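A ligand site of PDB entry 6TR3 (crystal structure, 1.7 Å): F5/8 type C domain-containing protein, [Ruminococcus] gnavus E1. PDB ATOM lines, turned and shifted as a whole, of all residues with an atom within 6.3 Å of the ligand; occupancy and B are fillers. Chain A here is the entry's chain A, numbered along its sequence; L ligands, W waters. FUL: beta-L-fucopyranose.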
ATOM      1  N   PHE A  43      40.157 -13.346 -25.328  1.00  0.00           N
ATOM      2  CA  PHE A  43      38.818 -13.892 -25.170  1.00  0.00           C
ATOM      3  C   PHE A  43      39.034 -15.378 -24.953  1.00  0.00           C
ATOM      4  O   PHE A  43      39.975 -15.975 -25.479  1.00  0.00           O
ATOM      5  CB  PHE A  43      38.016 -13.675 -26.469  1.00  0.00           C
ATOM      6  CG  PHE A  43      36.661 -13.031 -26.296  1.00  0.00           C
ATOM      7  CD1 PHE A  43      35.882 -13.235 -25.176  1.00  0.00           C
ATOM      8  CD2 PHE A  43      36.139 -12.250 -27.329  1.00  0.00           C
ATOM      9  CE1 PHE A  43      34.624 -12.657 -25.073  1.00  0.00           C
ATOM     10  CE2 PHE A  43      34.885 -11.680 -27.232  1.00  0.00           C
ATOM     11  CZ  PHE A  43      34.121 -11.881 -26.084  1.00  0.00           C
ATOM     12  N   HIS A  45      36.359 -18.521 -25.227  1.00  0.00           N
ATOM     13  CA  HIS A  45      35.093 -19.164 -25.498  1.00  0.00           C
ATOM     14  C   HIS A  45      35.265 -20.653 -25.203  1.00  0.00           C
ATOM     15  O   HIS A  45      36.159 -21.316 -25.738  1.00  0.00           O
ATOM     16  CB  HIS A  45      34.663 -18.969 -26.952  1.00  0.00           C
ATOM     17  CG  HIS A  45      34.079 -17.621 -27.232  1.00  0.00           C
ATOM     18  ND1 HIS A  45      34.832 -16.471 -27.242  1.00  0.00           N
ATOM     19  CD2 HIS A  45      32.800 -17.248 -27.534  1.00  0.00           C
ATOM     20  CE1 HIS A  45      34.040 -15.439 -27.527  1.00  0.00           C
ATOM     21  NE2 HIS A  45      32.806 -15.886 -27.712  1.00  0.00           N
ATOM     22  N   GLU A  55      28.889 -23.266 -33.474  1.00  0.00           N
ATOM     23  CA  GLU A  55      29.172 -21.918 -32.972  1.00  0.00           C
ATOM     24  C   GLU A  55      28.115 -21.338 -32.052  1.00  0.00           C
ATOM     25  O   GLU A  55      28.439 -20.649 -31.066  1.00  0.00           O
ATOM     26  CB  GLU A  55      29.467 -20.960 -34.129  1.00  0.00           C
ATOM     27  CG  GLU A  55      30.855 -21.165 -34.712  1.00  0.00           C
ATOM     28  CD  GLU A  55      31.957 -20.723 -33.768  1.00  0.00           C
ATOM     29  OE1 GLU A  55      32.039 -19.505 -33.514  1.00  0.00           O
ATOM     30  OE2 GLU A  55      32.748 -21.588 -33.348  1.00  0.00           O
ATOM     31  N   TRP A  56      26.847 -21.530 -32.419  1.00  0.00           N
ATOM     32  CA  TRP A  56      25.696 -21.175 -31.603  1.00  0.00           C
ATOM     33  C   TRP A  56      24.976 -22.466 -31.242  1.00  0.00           C
ATOM     34  O   TRP A  56      24.548 -23.188 -32.143  1.00  0.00           O
ATOM     35  CB  TRP A  56      24.738 -20.260 -32.405  1.00  0.00           C
ATOM     36  CG  TRP A  56      25.038 -18.784 -32.326  1.00  0.00           C
ATOM     37  CD1 TRP A  56      26.220 -18.180 -32.001  1.00  0.00           C
ATOM     38  CD2 TRP A  56      24.134 -17.723 -32.654  1.00  0.00           C
ATOM     39  NE1 TRP A  56      26.094 -16.817 -32.049  1.00  0.00           N
ATOM     40  CE2 TRP A  56      24.821 -16.513 -32.462  1.00  0.00           C
ATOM     41  CE3 TRP A  56      22.795 -17.682 -33.094  1.00  0.00           C
ATOM     42  CZ2 TRP A  56      24.212 -15.269 -32.683  1.00  0.00           C
ATOM     43  CZ3 TRP A  56      22.198 -16.454 -33.300  1.00  0.00           C
ATOM     44  CH2 TRP A  56      22.903 -15.262 -33.088  1.00  0.00           C
ATOM     45  N   THR A  95      33.725 -16.565 -21.267  1.00  0.00           N
ATOM     46  CA  THR A  95      32.333 -16.856 -21.515  1.00  0.00           C
ATOM     47  C   THR A  95      31.789 -17.779 -20.415  1.00  0.00           C
ATOM     48  O   THR A  95      31.756 -19.024 -20.570  1.00  0.00           O
ATOM     49  CB  THR A  95      32.095 -17.511 -22.907  1.00  0.00           C
ATOM     50  OG1 THR A  95      32.701 -18.804 -22.946  1.00  0.00           O
ATOM     51  CG2 THR A  95      32.620 -16.641 -24.026  1.00  0.00           C
ATOM     52  N   HIS A  98      27.226 -18.780 -22.560  1.00  0.00           N
ATOM     53  CA  HIS A  98      26.936 -18.412 -23.933  1.00  0.00           C
ATOM     54  C   HIS A  98      25.421 -18.444 -24.164  1.00  0.00           C
ATOM     55  O   HIS A  98      24.648 -18.586 -23.200  1.00  0.00           O
ATOM     56  CB  HIS A  98      27.740 -19.277 -24.920  1.00  0.00           C
ATOM     57  CG  HIS A  98      28.030 -18.604 -26.228  1.00  0.00           C
ATOM     58  ND1 HIS A  98      27.325 -18.879 -27.387  1.00  0.00           N
ATOM     59  CD2 HIS A  98      28.935 -17.654 -26.555  1.00  0.00           C
ATOM     60  CE1 HIS A  98      27.792 -18.124 -28.367  1.00  0.00           C
ATOM     61  NE2 HIS A  98      28.765 -17.365 -27.886  1.00  0.00           N
ATOM     62  N   HIS A  99      24.998 -18.295 -25.417  1.00  0.00           N
ATOM     63  CA  HIS A  99      23.591 -18.183 -25.786  1.00  0.00           C
ATOM     64  C   HIS A  99      22.809 -19.437 -25.378  1.00  0.00           C
ATOM     65  O   HIS A  99      21.644 -19.361 -25.012  1.00  0.00           O
ATOM     66  CB  HIS A  99      23.417 -17.992 -27.291  1.00  0.00           C
ATOM     67  CG  HIS A  99      24.069 -16.770 -27.846  1.00  0.00           C
ATOM     68  ND1 HIS A  99      24.203 -15.613 -27.124  1.00  0.00           N
ATOM     69  CD2 HIS A  99      24.594 -16.526 -29.072  1.00  0.00           C
ATOM     70  CE1 HIS A  99      24.795 -14.703 -27.880  1.00  0.00           C
ATOM     71  NE2 HIS A  99      25.046 -15.236 -29.063  1.00  0.00           N
ATOM     72  N   TYR A 146      31.787 -12.483 -19.599  1.00  0.00           N
ATOM     73  CA  TYR A 146      30.800 -12.554 -20.676  1.00  0.00           C
ATOM     74  C   TYR A 146      29.654 -13.420 -20.164  1.00  0.00           C
ATOM     75  O   TYR A 146      29.847 -14.569 -19.776  1.00  0.00           O
ATOM     76  CB  TYR A 146      31.456 -13.097 -21.922  1.00  0.00           C
ATOM     77  CG  TYR A 146      30.586 -13.425 -23.118  1.00  0.00           C
ATOM     78  CD1 TYR A 146      29.604 -14.380 -23.060  1.00  0.00           C
ATOM     79  CD2 TYR A 146      30.834 -12.799 -24.344  1.00  0.00           C
ATOM     80  CE1 TYR A 146      28.852 -14.688 -24.196  1.00  0.00           C
ATOM     81  CE2 TYR A 146      30.086 -13.087 -25.466  1.00  0.00           C
ATOM     82  CZ  TYR A 146      29.112 -14.038 -25.389  1.00  0.00           C
ATOM     83  OH  TYR A 146      28.432 -14.293 -26.552  1.00  0.00           O
ATOM     84  N   SER A 148      25.812 -14.109 -21.507  1.00  0.00           N
ATOM     85  CA  SER A 148      24.883 -13.877 -22.597  1.00  0.00           C
ATOM     86  C   SER A 148      23.497 -13.473 -22.090  1.00  0.00           C
ATOM     87  O   SER A 148      22.882 -14.204 -21.311  1.00  0.00           O
ATOM     88  CB  SER A 148      24.764 -15.115 -23.481  1.00  0.00           C
ATOM     89  OG  SER A 148      23.770 -14.886 -24.474  1.00  0.00           O
ATOM     90  N   TRP A 203      30.706  -8.113 -20.420  1.00  0.00           N
ATOM     91  CA  TRP A 203      30.216  -8.261 -21.786  1.00  0.00           C
ATOM     92  C   TRP A 203      28.771  -8.762 -21.782  1.00  0.00           C
ATOM     93  O   TRP A 203      28.471  -9.886 -21.332  1.00  0.00           O
ATOM     94  CB  TRP A 203      31.092  -9.251 -22.562  1.00  0.00           C
ATOM     95  CG  TRP A 203      31.953  -8.683 -23.679  1.00  0.00           C
ATOM     96  CD1 TRP A 203      33.048  -7.876 -23.553  1.00  0.00           C
ATOM     97  CD2 TRP A 203      31.806  -8.946 -25.083  1.00  0.00           C
ATOM     98  NE1 TRP A 203      33.581  -7.603 -24.793  1.00  0.00           N
ATOM     99  CE2 TRP A 203      32.839  -8.257 -25.741  1.00  0.00           C
ATOM    100  CE3 TRP A 203      30.896  -9.701 -25.835  1.00  0.00           C
ATOM    101  CZ2 TRP A 203      32.987  -8.293 -27.112  1.00  0.00           C
ATOM    102  CZ3 TRP A 203      31.044  -9.729 -27.217  1.00  0.00           C
ATOM    103  CH2 TRP A 203      32.082  -9.028 -27.849  1.00  0.00           C
ATOM    104  N   ASP A 205      26.679  -8.640 -24.713  1.00  0.00           N
ATOM    105  CA  ASP A 205      26.386  -8.453 -26.129  1.00  0.00           C
ATOM    106  C   ASP A 205      24.986  -8.883 -26.501  1.00  0.00           C
ATOM    107  O   ASP A 205      24.485  -9.917 -26.047  1.00  0.00           O
ATOM    108  CB  ASP A 205      27.389  -9.128 -27.044  1.00  0.00           C
ATOM    109  CG  ASP A 205      27.162  -8.794 -28.505  1.00  0.00           C
ATOM    110  OD1 ASP A 205      27.423  -7.638 -28.956  1.00  0.00           O
ATOM    111  OD2 ASP A 205      26.689  -9.694 -29.208  1.00  0.00           O
ATOM    112  N   GLY A 206      24.358  -8.079 -27.357  1.00  0.00           N
ATOM    113  CA  GLY A 206      22.954  -8.255 -27.695  1.00  0.00           C
ATOM    114  C   GLY A 206      22.655  -9.165 -28.875  1.00  0.00           C
ATOM    115  O   GLY A 206      21.528  -9.213 -29.329  1.00  0.00           O
ATOM    116  N   ALA A 207      23.644  -9.910 -29.387  1.00  0.00           N
ATOM    117  CA  ALA A 207      23.371 -10.875 -30.450  1.00  0.00           C
ATOM    118  C   ALA A 207      22.292 -11.875 -30.020  1.00  0.00           C
ATOM    119  O   ALA A 207      22.332 -12.446 -28.917  1.00  0.00           O
ATOM    120  CB  ALA A 207      24.624 -11.599 -30.909  1.00  0.00           C
ATOM    121  N   LYS A 208      21.305 -12.063 -30.902  1.00  0.00           N
ATOM    122  CA  LYS A 208      20.119 -12.793 -30.588  1.00  0.00           C
ATOM    123  C   LYS A 208      19.515 -13.404 -31.851  1.00  0.00           C
ATOM    124  O   LYS A 208      19.449 -12.725 -32.858  1.00  0.00           O
ATOM    125  CB  LYS A 208      19.123 -11.831 -29.938  1.00  0.00           C
ATOM    126  CG  LYS A 208      17.961 -12.523 -29.276  1.00  0.00           C
ATOM    127  CD  LYS A 208      16.912 -11.534 -28.805  1.00  0.00           C
ATOM    128  CE  LYS A 208      15.754 -12.247 -28.149  1.00  0.00           C
ATOM    129  NZ  LYS A 208      14.908 -11.286 -27.404  1.00  0.00           N
ATOM    130  N   GLU A 257      34.298  -8.193 -36.942  1.00  0.00           N
ATOM    131  CA  GLU A 257      35.026  -9.244 -36.216  1.00  0.00           C
ATOM    132  C   GLU A 257      36.360  -9.596 -36.857  1.00  0.00           C
ATOM    133  O   GLU A 257      36.861 -10.693 -36.665  1.00  0.00           O
ATOM    134  CB  GLU A 257      34.158 -10.480 -36.078  1.00  0.00           C
ATOM    135  CG  GLU A 257      32.875 -10.243 -35.313  1.00  0.00           C
ATOM    136  CD  GLU A 257      31.969 -11.460 -35.273  1.00  0.00           C
ATOM    137  OE1 GLU A 257      32.051 -12.320 -36.202  1.00  0.00           O
ATOM    138  OE2 GLU A 257      31.188 -11.560 -34.295  1.00  0.00           O
ATOM    139  N   ASP A 302      37.201  -7.103 -31.539  1.00  0.00           N
ATOM    140  CA  ASP A 302      37.227  -8.520 -31.185  1.00  0.00           C
ATOM    141  C   ASP A 302      37.498  -9.385 -32.414  1.00  0.00           C
ATOM    142  O   ASP A 302      37.011  -9.088 -33.506  1.00  0.00           O
ATOM    143  CB  ASP A 302      35.944  -8.950 -30.452  1.00  0.00           C
ATOM    144  CG  ASP A 302      34.675  -8.810 -31.285  1.00  0.00           C
ATOM    145  OD1 ASP A 302      34.511  -7.875 -32.097  1.00  0.00           O
ATOM    146  OD2 ASP A 302      33.788  -9.699 -31.099  1.00  0.00           O
ATOM    147  N   TRP A 309      34.694 -18.918 -32.929  1.00  0.00           N
ATOM    148  CA  TRP A 309      34.883 -18.566 -31.533  1.00  0.00           C
ATOM    149  C   TRP A 309      35.193 -19.782 -30.669  1.00  0.00           C
ATOM    150  O   TRP A 309      35.948 -19.694 -29.707  1.00  0.00           O
ATOM    151  CB  TRP A 309      33.661 -17.810 -30.976  1.00  0.00           C
ATOM    152  CG  TRP A 309      33.406 -16.492 -31.683  1.00  0.00           C
ATOM    153  CD1 TRP A 309      32.364 -16.193 -32.528  1.00  0.00           C
ATOM    154  CD2 TRP A 309      34.187 -15.297 -31.577  1.00  0.00           C
ATOM    155  NE1 TRP A 309      32.480 -14.896 -32.975  1.00  0.00           N
ATOM    156  CE2 TRP A 309      33.583 -14.321 -32.397  1.00  0.00           C
ATOM    157  CE3 TRP A 309      35.365 -14.961 -30.877  1.00  0.00           C
ATOM    158  CZ2 TRP A 309      34.112 -13.033 -32.524  1.00  0.00           C
ATOM    159  CZ3 TRP A 309      35.888 -13.672 -31.012  1.00  0.00           C
ATOM    160  CH2 TRP A 309      35.253 -12.722 -31.824  1.00  0.00           C
ATOM    161  N   PHE A 310      34.537 -20.907 -30.966  1.00  0.00           N
ATOM    162  CA  PHE A 310      34.780 -22.146 -30.262  1.00  0.00           C
ATOM    163  C   PHE A 310      35.705 -23.034 -31.037  1.00  0.00           C
ATOM    164  O   PHE A 310      35.614 -23.116 -32.273  1.00  0.00           O
ATOM    165  CB  PHE A 310      33.460 -22.859 -30.015  1.00  0.00           C
ATOM    166  CG  PHE A 310      32.602 -22.161 -29.022  1.00  0.00           C
ATOM    167  CD1 PHE A 310      32.730 -22.419 -27.675  1.00  0.00           C
ATOM    168  CD2 PHE A 310      31.680 -21.205 -29.432  1.00  0.00           C
ATOM    169  CE1 PHE A 310      31.929 -21.770 -26.755  1.00  0.00           C
ATOM    170  CE2 PHE A 310      30.880 -20.556 -28.512  1.00  0.00           C
ATOM    171  CZ  PHE A 310      31.006 -20.829 -27.166  1.00  0.00           C
HETATM  172  C1  FUL L   1      28.346 -12.645 -29.726  1.00  0.00           C
HETATM  173  C2  FUL L   1      28.010 -14.098 -30.039  1.00  0.00           C
HETATM  174  O2  FUL L   1      26.850 -14.173 -30.884  1.00  0.00           O
HETATM  175  C3  FUL L   1      29.156 -14.843 -30.716  1.00  0.00           C
HETATM  176  O3  FUL L   1      28.833 -16.241 -30.695  1.00  0.00           O
HETATM  177  C4  FUL L   1      30.467 -14.581 -29.971  1.00  0.00           C
HETATM  178  O4  FUL L   1      30.365 -15.156 -28.664  1.00  0.00           O
HETATM  179  C5  FUL L   1      30.734 -13.087 -29.886  1.00  0.00           C
HETATM  180  C6  FUL L   1      32.074 -12.801 -29.204  1.00  0.00           C
HETATM  181  O5  FUL L   1      29.658 -12.474 -29.160  1.00  0.00           O
HETATM  182  O1  FUL L   1      27.363 -12.196 -28.774  1.00  0.00           O
HETATM  183  O   HOH W   1      27.259 -12.572 -32.919  1.00  0.00           O
HETATM  184  O   HOH W   2      30.179 -18.586 -31.469  1.00  0.00           O
HETATM  185  O   HOH W   3      26.306 -12.451 -25.808  1.00  0.00           O
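An oxygen (O4) of the ligand is in hydrogen-bond range of the side-chain hydroxyl (OH) of Tyr 146. An oxygen (O2) of the ligand lies within hydrogen-bond range of a ring nitrogen (NE2) of His 99 (2.8 Å). The indole nitrogen (NE1) of Trp 56 is in hydrogen-bond range of an oxygen (O2) of the ligand, at 3.0 Å. O4 of the ligand lies within hydrogen-bond range of NE2 of His 45. A ring nitrogen (NE2) of His 98 is in hydrogen-bond range of an oxygen (O4) of the ligand (2.8 Å). OD2 of Asp 205 sits at hydrogen-bond distance from O1 of the ligand (2.6 Å).
Water W2 bridges O of Glu 55 (2.7 Å) and O3 of the ligand (2.8 Å). Water W3 lies within hydrogen-bond range of the side-chain hydroxyl (OH) of Tyr 146, the backbone carbonyl oxygen (O) of Asp 205 and an oxygen (O1) of the ligand.
Residues that only touch the ligand: Phe 43 (3.6 Å), Trp 203 (3.6 Å), Ala 207 (3.4 Å) and Trp 309 (3.6 Å). Hydrophobic or aromatic side chains within 4 Å of the ligand: Phe 43, His 45, Trp 56, His 98, His 99, Tyr 146, Trp 203, Ala 207 and Trp 309. Of the 18 residues printed, 10 come within 4 Å of the ligand. The nearest printed residue that does not touch the ligand is Asp 302 (4.02 Å).
The backbone NH of Trp 309 lies within hydrogen-bond range of the side-chain carboxylate of Glu 55, 2.8 Å away. A ring nitrogen (ND1) of His 99 sits at hydrogen-bond distance from the side-chain hydroxyl (OG) of Ser 148 (2.8 Å). The side-chain hydroxyl of Tyr 146 is in hydrogen-bond range of a ring nitrogen (NE2) of His 98 (3.4 Å). The side-chain carboxylate (OD2) of Asp 205 lies within hydrogen-bond range of the backbone NH (N) of Ala 207, at 3.1 Å.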
